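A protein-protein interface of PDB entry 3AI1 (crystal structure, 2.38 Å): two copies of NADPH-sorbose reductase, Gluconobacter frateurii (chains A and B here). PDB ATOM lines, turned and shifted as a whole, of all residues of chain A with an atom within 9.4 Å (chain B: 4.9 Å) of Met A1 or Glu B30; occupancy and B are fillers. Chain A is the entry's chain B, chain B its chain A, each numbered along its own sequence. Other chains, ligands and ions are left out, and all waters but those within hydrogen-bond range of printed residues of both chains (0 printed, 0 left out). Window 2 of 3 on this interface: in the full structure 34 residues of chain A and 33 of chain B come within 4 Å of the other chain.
Among the printed residues, merely in contact across the chains: Met A1 with Met B3, Asn A235 with Met B1, Asn A235 with Phe B239, Val A238 with Met B1, Phe A239 with Asn B235 and Phe A239 with Phe B239.
Of chain B, only Met B1, Met B3 and Glu B30 come within 4 Å of Met A1. No residue of chain A comes within 4 Å of Gly B31. Of the printed residues of chain B, Glu A30 touches Met B1. Printed residues of chain A within 4 Å of Asn B235: Phe A239 and Arg A244. Printed residues of chain A within 4 Å of Met B3: Met A1 (3.6 Å). Of the printed residues of chain A, Met B1 touches Met A1 (2.9 Å), Glu A30 (2.9 Å), Asn A235 (3.7 Å) and Val A238 (3.7 Å). Printed residues of chain B within 4 Å of Phe A239: Asn B235 (3.97 Å) and Phe B239 (3.8 Å). The nearest residue of chain A that does not touch Glu B30 is Asp A2 (5.4 Å).
Met A1 touches Met B3, but with the chains exchanged Met A3 does not touch Met B1 (4.04 Å). Met A1 touches Glu B30, and with the chains exchanged Glu A30 touches Met B1. Asn A235 touches Phe B239, and with the chains exchanged Phe A239 touches Asn B235. Phe A239 touches its own counterpart, Phe B239. Positions printed for both chains: 1, 3, 5, 30, 235, 238 and 239. Of the 10 pairs that touch across the chains among the printed residues, 6 have their exchanged pair printed and touching as well.
Of the 14 printed residues of chain B, 5 touch a printed residue of chain A. Hydrophobic or aromatic side chains of chain B within 4 Å of the printed part of chain A: Met B1, Met B3 and Phe B239. Hydrophobic or aromatic side chains of chain A that line the printed part of chain B: Met A1, Val A238 and Phe A239. Among the printed residues, 10 pairs touch across the chains. Among the printed residues, no Asp or Glu carboxylate lies within 4 Å of a Lys or Arg side-chain nitrogen of the other chain.
N of Met A1 is in hydrogen-bond range of O of Met B1, at 2.9 Å. The side-chain carboxylate (OE1) of Glu B30 lies within hydrogen-bond range of the backbone NH (N) of Met A1 (3.1 Å). OE2 of Glu A30 sits at hydrogen-bond distance from N of Met B1, 2.9 Å away. The backbone carbonyl oxygen of Arg A244 lies within hydrogen-bond range of the side-chain amide nitrogen of Asn B235, at 2.9 Å.
The backbone carbonyl oxygen (O) of Phe A239 sits at hydrogen-bond distance from the side-chain hydroxyl (OG) of Ser A242 (2.6 Å). The side-chain carboxylate (OE2) of Glu A243 is in salt-bridge range of the guanidinium group (NH1) of Arg A244. O of Asp A2 lies within hydrogen-bond range of NH1 of Arg A244, 2.7 Å away. N of Arg A244 sits at hydrogen-bond distance from OG of Ser A242 (3.0 Å).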
ATOM      1  N   MET A   1     -23.014  25.741   6.209  1.00  0.00           N
ATOM      2  CA  MET A   1     -21.897  25.003   5.559  1.00  0.00           C
ATOM      3  C   MET A   1     -20.671  25.914   5.495  1.00  0.00           C
ATOM      4  O   MET A   1     -20.750  27.032   4.990  1.00  0.00           O
ATOM      5  CB  MET A   1     -22.330  24.536   4.161  1.00  0.00           C
ATOM      6  CG  MET A   1     -21.358  23.594   3.463  1.00  0.00           C
ATOM      7  SD  MET A   1     -21.987  22.823   1.952  1.00  0.00           S
ATOM      8  CE  MET A   1     -22.608  24.192   0.987  1.00  0.00           C
ATOM      9  N   ASP A   2     -19.554  25.445   6.046  1.00  0.00           N
ATOM     10  CA  ASP A   2     -18.300  26.207   6.012  1.00  0.00           C
ATOM     11  C   ASP A   2     -17.651  26.045   4.646  1.00  0.00           C
ATOM     12  O   ASP A   2     -17.315  24.933   4.232  1.00  0.00           O
ATOM     13  CB  ASP A   2     -17.350  25.765   7.141  1.00  0.00           C
ATOM     14  CG  ASP A   2     -15.980  26.473   7.097  1.00  0.00           C
ATOM     15  OD1 ASP A   2     -15.011  25.902   7.659  1.00  0.00           O
ATOM     16  OD2 ASP A   2     -15.855  27.585   6.514  1.00  0.00           O
ATOM     17  N   MET A   3     -17.477  27.166   3.955  1.00  0.00           N
ATOM     18  CA  MET A   3     -16.932  27.183   2.604  1.00  0.00           C
ATOM     19  C   MET A   3     -15.417  26.993   2.555  1.00  0.00           C
ATOM     20  O   MET A   3     -14.863  26.656   1.499  1.00  0.00           O
ATOM     21  CB  MET A   3     -17.314  28.490   1.906  1.00  0.00           C
ATOM     22  CG  MET A   3     -18.797  28.667   1.631  1.00  0.00           C
ATOM     23  SD  MET A   3     -19.447  27.498   0.423  1.00  0.00           S
ATOM     24  CE  MET A   3     -20.140  26.256   1.496  1.00  0.00           C
ATOM     25  N   GLY A   4     -14.758  27.223   3.692  1.00  0.00           N
ATOM     26  CA  GLY A   4     -13.301  27.083   3.817  1.00  0.00           C
ATOM     27  C   GLY A   4     -12.527  28.071   2.968  1.00  0.00           C
ATOM     28  O   GLY A   4     -11.428  27.781   2.497  1.00  0.00           O
ATOM     29  N   ILE A   5     -13.105  29.252   2.799  1.00  0.00           N
ATOM     30  CA  ILE A   5     -12.621  30.246   1.849  1.00  0.00           C
ATOM     31  C   ILE A   5     -11.883  31.377   2.558  1.00  0.00           C
ATOM     32  O   ILE A   5     -11.154  32.142   1.926  1.00  0.00           O
ATOM     33  CB  ILE A   5     -13.807  30.780   0.981  1.00  0.00           C
ATOM     34  CG1 ILE A   5     -14.253  29.706  -0.011  1.00  0.00           C
ATOM     35  CG2 ILE A   5     -13.447  32.051   0.233  1.00  0.00           C
ATOM     36  CD1 ILE A   5     -15.481  30.088  -0.810  1.00  0.00           C
ATOM     37  N   GLU A  30     -17.491  35.430   2.942  1.00  0.00           N
ATOM     38  CA  GLU A  30     -16.801  34.212   3.365  1.00  0.00           C
ATOM     39  C   GLU A  30     -15.348  34.452   3.791  1.00  0.00           C
ATOM     40  O   GLU A  30     -14.589  33.499   3.969  1.00  0.00           O
ATOM     41  CB  GLU A  30     -16.859  33.149   2.257  1.00  0.00           C
ATOM     42  CG  GLU A  30     -18.264  32.593   1.962  1.00  0.00           C
ATOM     43  CD  GLU A  30     -18.963  31.980   3.172  1.00  0.00           C
ATOM     44  OE1 GLU A  30     -18.324  31.216   3.933  1.00  0.00           O
ATOM     45  OE2 GLU A  30     -20.173  32.256   3.349  1.00  0.00           O
ATOM     46  N   ASN A 235     -23.998  33.222  -5.104  1.00  0.00           N
ATOM     47  CA  ASN A 235     -23.980  32.026  -4.273  1.00  0.00           C
ATOM     48  C   ASN A 235     -23.328  30.827  -4.947  1.00  0.00           C
ATOM     49  O   ASN A 235     -22.559  30.096  -4.314  1.00  0.00           O
ATOM     50  CB  ASN A 235     -25.401  31.671  -3.844  1.00  0.00           C
ATOM     51  CG  ASN A 235     -25.984  32.670  -2.858  1.00  0.00           C
ATOM     52  OD1 ASN A 235     -25.255  33.393  -2.172  1.00  0.00           O
ATOM     53  ND2 ASN A 235     -27.312  32.709  -2.778  1.00  0.00           N
ATOM     54  N   VAL A 238     -19.360  31.265  -5.374  1.00  0.00           N
ATOM     55  CA  VAL A 238     -18.710  31.044  -4.085  1.00  0.00           C
ATOM     56  C   VAL A 238     -18.601  29.552  -3.739  1.00  0.00           C
ATOM     57  O   VAL A 238     -17.528  29.083  -3.358  1.00  0.00           O
ATOM     58  CB  VAL A 238     -19.428  31.831  -2.951  1.00  0.00           C
ATOM     59  CG1 VAL A 238     -18.862  31.485  -1.582  1.00  0.00           C
ATOM     60  CG2 VAL A 238     -19.326  33.326  -3.210  1.00  0.00           C
ATOM     61  N   PHE A 239     -19.702  28.818  -3.895  1.00  0.00           N
ATOM     62  CA  PHE A 239     -19.746  27.386  -3.569  1.00  0.00           C
ATOM     63  C   PHE A 239     -18.814  26.559  -4.461  1.00  0.00           C
ATOM     64  O   PHE A 239     -18.133  25.651  -3.983  1.00  0.00           O
ATOM     65  CB  PHE A 239     -21.183  26.864  -3.656  1.00  0.00           C
ATOM     66  CG  PHE A 239     -21.289  25.362  -3.637  1.00  0.00           C
ATOM     67  CD1 PHE A 239     -21.235  24.661  -2.436  1.00  0.00           C
ATOM     68  CD2 PHE A 239     -21.443  24.649  -4.825  1.00  0.00           C
ATOM     69  CE1 PHE A 239     -21.337  23.276  -2.417  1.00  0.00           C
ATOM     70  CE2 PHE A 239     -21.540  23.268  -4.816  1.00  0.00           C
ATOM     71  CZ  PHE A 239     -21.488  22.574  -3.611  1.00  0.00           C
ATOM     72  N   LEU A 240     -18.783  26.887  -5.751  1.00  0.00           N
ATOM     73  CA  LEU A 240     -17.918  26.207  -6.717  1.00  0.00           C
ATOM     74  C   LEU A 240     -16.426  26.488  -6.524  1.00  0.00           C
ATOM     75  O   LEU A 240     -15.578  25.727  -6.998  1.00  0.00           O
ATOM     76  CB  LEU A 240     -18.329  26.579  -8.135  1.00  0.00           C
ATOM     77  CG  LEU A 240     -19.019  25.555  -9.037  1.00  0.00           C
ATOM     78  CD1 LEU A 240     -20.012  24.646  -8.304  1.00  0.00           C
ATOM     79  CD2 LEU A 240     -19.700  26.300 -10.154  1.00  0.00           C
ATOM     80  N   SER A 242     -15.234  26.838  -3.462  1.00  0.00           N
ATOM     81  CA  SER A 242     -15.050  26.483  -2.063  1.00  0.00           C
ATOM     82  C   SER A 242     -14.413  25.112  -1.925  1.00  0.00           C
ATOM     83  O   SER A 242     -14.313  24.363  -2.906  1.00  0.00           O
ATOM     84  CB  SER A 242     -16.400  26.494  -1.344  1.00  0.00           C
ATOM     85  OG  SER A 242     -17.128  25.302  -1.592  1.00  0.00           O
ATOM     86  N   GLU A 243     -13.994  24.782  -0.704  1.00  0.00           N
ATOM     87  CA  GLU A 243     -13.467  23.450  -0.415  1.00  0.00           C
ATOM     88  C   GLU A 243     -14.598  22.436  -0.203  1.00  0.00           C
ATOM     89  O   GLU A 243     -14.351  21.280   0.135  1.00  0.00           O
ATOM     90  CB  GLU A 243     -12.452  23.462   0.746  1.00  0.00           C
ATOM     91  CG  GLU A 243     -12.959  24.046   2.063  1.00  0.00           C
ATOM     92  CD  GLU A 243     -11.941  23.959   3.223  1.00  0.00           C
ATOM     93  OE1 GLU A 243     -10.722  24.190   2.999  1.00  0.00           O
ATOM     94  OE2 GLU A 243     -12.378  23.680   4.369  1.00  0.00           O
ATOM     95  N   ARG A 244     -15.839  22.872  -0.425  1.00  0.00           N
ATOM     96  CA  ARG A 244     -16.984  21.962  -0.442  1.00  0.00           C
ATOM     97  C   ARG A 244     -17.308  21.434  -1.850  1.00  0.00           C
ATOM     98  O   ARG A 244     -18.192  20.597  -1.998  1.00  0.00           O
ATOM     99  CB  ARG A 244     -18.238  22.626   0.159  1.00  0.00           C
ATOM    100  CG  ARG A 244     -18.103  23.138   1.604  1.00  0.00           C
ATOM    101  CD  ARG A 244     -18.219  22.042   2.686  1.00  0.00           C
ATOM    102  NE  ARG A 244     -17.017  21.221   2.813  1.00  0.00           N
ATOM    103  CZ  ARG A 244     -15.827  21.662   3.224  1.00  0.00           C
ATOM    104  NH1 ARG A 244     -15.646  22.938   3.553  1.00  0.00           N
ATOM    105  NH2 ARG A 244     -14.804  20.821   3.301  1.00  0.00           N
ATOM    106  N   ALA A 245     -16.606  21.924  -2.873  1.00  0.00           N
ATOM    107  CA  ALA A 245     -16.878  21.530  -4.270  1.00  0.00           C
ATOM    108  C   ALA A 245     -15.662  20.904  -4.950  1.00  0.00           C
ATOM    109  O   ALA A 245     -15.391  21.159  -6.122  1.00  0.00           O
ATOM    110  CB  ALA A 245     -17.380  22.726  -5.081  1.00  0.00           C
ATOM    111  N   MET B   1     -21.362  29.837   4.542  1.00  0.00           N
ATOM    112  CA  MET B   1     -22.671  30.096   3.882  1.00  0.00           C
ATOM    113  C   MET B   1     -23.794  29.444   4.680  1.00  0.00           C
ATOM    114  O   MET B   1     -23.708  28.261   5.026  1.00  0.00           O
ATOM    115  CB  MET B   1     -22.650  29.566   2.441  1.00  0.00           C
ATOM    116  CG  MET B   1     -23.768  30.096   1.551  1.00  0.00           C
ATOM    117  SD  MET B   1     -23.593  29.669  -0.199  1.00  0.00           S
ATOM    118  CE  MET B   1     -22.426  30.912  -0.736  1.00  0.00           C
ATOM    119  N   MET B   3     -27.156  27.780   4.731  1.00  0.00           N
ATOM    120  CA  MET B   3     -27.974  27.015   3.789  1.00  0.00           C
ATOM    121  C   MET B   3     -29.461  27.312   3.910  1.00  0.00           C
ATOM    122  O   MET B   3     -30.217  27.128   2.954  1.00  0.00           O
ATOM    123  CB  MET B   3     -27.727  25.515   3.973  1.00  0.00           C
ATOM    124  CG  MET B   3     -26.748  24.886   2.986  1.00  0.00           C
ATOM    125  SD  MET B   3     -25.442  25.979   2.399  1.00  0.00           S
ATOM    126  CE  MET B   3     -25.970  26.308   0.734  1.00  0.00           C
ATOM    127  N   ILE B   5     -31.855  25.857   5.757  1.00  0.00           N
ATOM    128  CA  ILE B   5     -32.745  24.686   5.761  1.00  0.00           C
ATOM    129  C   ILE B   5     -32.961  24.049   7.138  1.00  0.00           C
ATOM    130  O   ILE B   5     -33.530  22.960   7.238  1.00  0.00           O
ATOM    131  CB  ILE B   5     -32.298  23.594   4.738  1.00  0.00           C
ATOM    132  CG1 ILE B   5     -30.854  23.143   5.013  1.00  0.00           C
ATOM    133  CG2 ILE B   5     -32.506  24.090   3.310  1.00  0.00           C
ATOM    134  CD1 ILE B   5     -30.363  22.016   4.142  1.00  0.00           C
ATOM    135  N   SER B   6     -32.516  24.724   8.197  1.00  0.00           N
ATOM    136  CA  SER B   6     -32.755  24.235   9.549  1.00  0.00           C
ATOM    137  C   SER B   6     -34.257  24.144   9.802  1.00  0.00           C
ATOM    138  O   SER B   6     -34.992  25.105   9.573  1.00  0.00           O
ATOM    139  CB  SER B   6     -32.091  25.138  10.589  1.00  0.00           C
ATOM    140  OG  SER B   6     -32.252  24.596  11.895  1.00  0.00           O
ATOM    141  N   GLY B  26     -25.440  15.088   5.433  1.00  0.00           N
ATOM    142  CA  GLY B  26     -25.236  16.444   4.933  1.00  0.00           C
ATOM    143  C   GLY B  26     -26.380  17.362   5.310  1.00  0.00           C
ATOM    144  O   GLY B  26     -26.166  18.502   5.730  1.00  0.00           O
ATOM    145  N   PHE B  27     -27.604  16.862   5.166  1.00  0.00           N
ATOM    146  CA  PHE B  27     -28.782  17.638   5.520  1.00  0.00           C
ATOM    147  C   PHE B  27     -28.936  17.780   7.034  1.00  0.00           C
ATOM    148  O   PHE B  27     -29.246  18.869   7.523  1.00  0.00           O
ATOM    149  CB  PHE B  27     -30.042  17.046   4.891  1.00  0.00           C
ATOM    150  CG  PHE B  27     -30.192  17.351   3.430  1.00  0.00           C
ATOM    151  CD1 PHE B  27     -30.001  16.361   2.477  1.00  0.00           C
ATOM    152  CD2 PHE B  27     -30.537  18.632   3.004  1.00  0.00           C
ATOM    153  CE1 PHE B  27     -30.149  16.647   1.119  1.00  0.00           C
ATOM    154  CE2 PHE B  27     -30.687  18.923   1.650  1.00  0.00           C
ATOM    155  CZ  PHE B  27     -30.488  17.931   0.709  1.00  0.00           C
ATOM    156  N   ALA B  28     -28.693  16.692   7.764  1.00  0.00           N
ATOM    157  CA  ALA B  28     -28.757  16.691   9.227  1.00  0.00           C
ATOM    158  C   ALA B  28     -27.763  17.677   9.845  1.00  0.00           C
ATOM    159  O   ALA B  28     -28.076  18.351  10.830  1.00  0.00           O
ATOM    160  CB  ALA B  28     -28.538  15.292   9.774  1.00  0.00           C
ATOM    161  N   LYS B  29     -26.578  17.765   9.249  1.00  0.00           N
ATOM    162  CA  LYS B  29     -25.569  18.743   9.646  1.00  0.00           C
ATOM    163  C   LYS B  29     -26.122  20.166   9.574  1.00  0.00           C
ATOM    164  O   LYS B  29     -25.811  21.001  10.415  1.00  0.00           O
ATOM    165  CB  LYS B  29     -24.336  18.610   8.752  1.00  0.00           C
ATOM    166  CG  LYS B  29     -23.101  19.330   9.255  1.00  0.00           C
ATOM    167  CD  LYS B  29     -21.855  18.764   8.596  1.00  0.00           C
ATOM    168  CE  LYS B  29     -20.632  19.633   8.860  1.00  0.00           C
ATOM    169  NZ  LYS B  29     -19.412  19.000   8.281  1.00  0.00           N
ATOM    170  N   GLU B  30     -26.954  20.425   8.571  1.00  0.00           N
ATOM    171  CA  GLU B  30     -27.509  21.754   8.347  1.00  0.00           C
ATOM    172  C   GLU B  30     -28.829  21.989   9.095  1.00  0.00           C
ATOM    173  O   GLU B  30     -29.511  22.992   8.872  1.00  0.00           O
ATOM    174  CB  GLU B  30     -27.652  22.022   6.846  1.00  0.00           C
ATOM    175  CG  GLU B  30     -26.342  21.917   6.067  1.00  0.00           C
ATOM    176  CD  GLU B  30     -25.335  23.002   6.423  1.00  0.00           C
ATOM    177  OE1 GLU B  30     -25.708  24.197   6.431  1.00  0.00           O
ATOM    178  OE2 GLU B  30     -24.159  22.666   6.678  1.00  0.00           O
ATOM    179  N   GLY B  31     -29.173  21.054   9.980  1.00  0.00           N
ATOM    180  CA  GLY B  31     -30.299  21.208  10.900  1.00  0.00           C
ATOM    181  C   GLY B  31     -31.633  20.696  10.390  1.00  0.00           C
ATOM    182  O   GLY B  31     -32.665  20.907  11.028  1.00  0.00           O
ATOM    183  N   ALA B  32     -31.613  20.024   9.241  1.00  0.00           N
ATOM    184  CA  ALA B  32     -32.823  19.473   8.645  1.00  0.00           C
ATOM    185  C   ALA B  32     -33.235  18.165   9.314  1.00  0.00           C
ATOM    186  O   ALA B  32     -32.384  17.363   9.697  1.00  0.00           O
ATOM    187  CB  ALA B  32     -32.621  19.265   7.152  1.00  0.00           C
ATOM    188  N   ASN B 235     -22.388  17.387  -0.335  1.00  0.00           N
ATOM    189  CA  ASN B 235     -22.276  18.849  -0.348  1.00  0.00           C
ATOM    190  C   ASN B 235     -23.132  19.478  -1.434  1.00  0.00           C
ATOM    191  O   ASN B 235     -23.838  20.452  -1.194  1.00  0.00           O
ATOM    192  CB  ASN B 235     -20.816  19.263  -0.558  1.00  0.00           C
ATOM    193  CG  ASN B 235     -19.914  18.896   0.624  1.00  0.00           C
ATOM    194  OD1 ASN B 235     -20.381  18.454   1.667  1.00  0.00           O
ATOM    195  ND2 ASN B 235     -18.613  19.084   0.452  1.00  0.00           N
ATOM    196  N   VAL B 238     -26.972  19.107  -0.827  1.00  0.00           N
ATOM    197  CA  VAL B 238     -27.357  20.056   0.211  1.00  0.00           C
ATOM    198  C   VAL B 238     -27.500  21.471  -0.350  1.00  0.00           C
ATOM    199  O   VAL B 238     -28.539  22.107  -0.179  1.00  0.00           O
ATOM    200  CB  VAL B 238     -26.333  20.077   1.395  1.00  0.00           C
ATOM    201  CG1 VAL B 238     -26.773  21.054   2.460  1.00  0.00           C
ATOM    202  CG2 VAL B 238     -26.159  18.694   2.000  1.00  0.00           C
ATOM    203  N   PHE B 239     -26.457  21.953  -1.021  1.00  0.00           N
ATOM    204  CA  PHE B 239     -26.461  23.301  -1.571  1.00  0.00           C
ATOM    205  C   PHE B 239     -27.627  23.530  -2.540  1.00  0.00           C
ATOM    206  O   PHE B 239     -28.272  24.578  -2.514  1.00  0.00           O
ATOM    207  CB  PHE B 239     -25.119  23.614  -2.246  1.00  0.00           C
ATOM    208  CG  PHE B 239     -25.113  24.914  -3.011  1.00  0.00           C
ATOM    209  CD1 PHE B 239     -24.875  26.116  -2.362  1.00  0.00           C
ATOM    210  CD2 PHE B 239     -25.356  24.930  -4.381  1.00  0.00           C
ATOM    211  CE1 PHE B 239     -24.879  27.320  -3.060  1.00  0.00           C
ATOM    212  CE2 PHE B 239     -25.360  26.125  -5.088  1.00  0.00           C
ATOM    213  CZ  PHE B 239     -25.122  27.328  -4.425  1.00  0.00           C
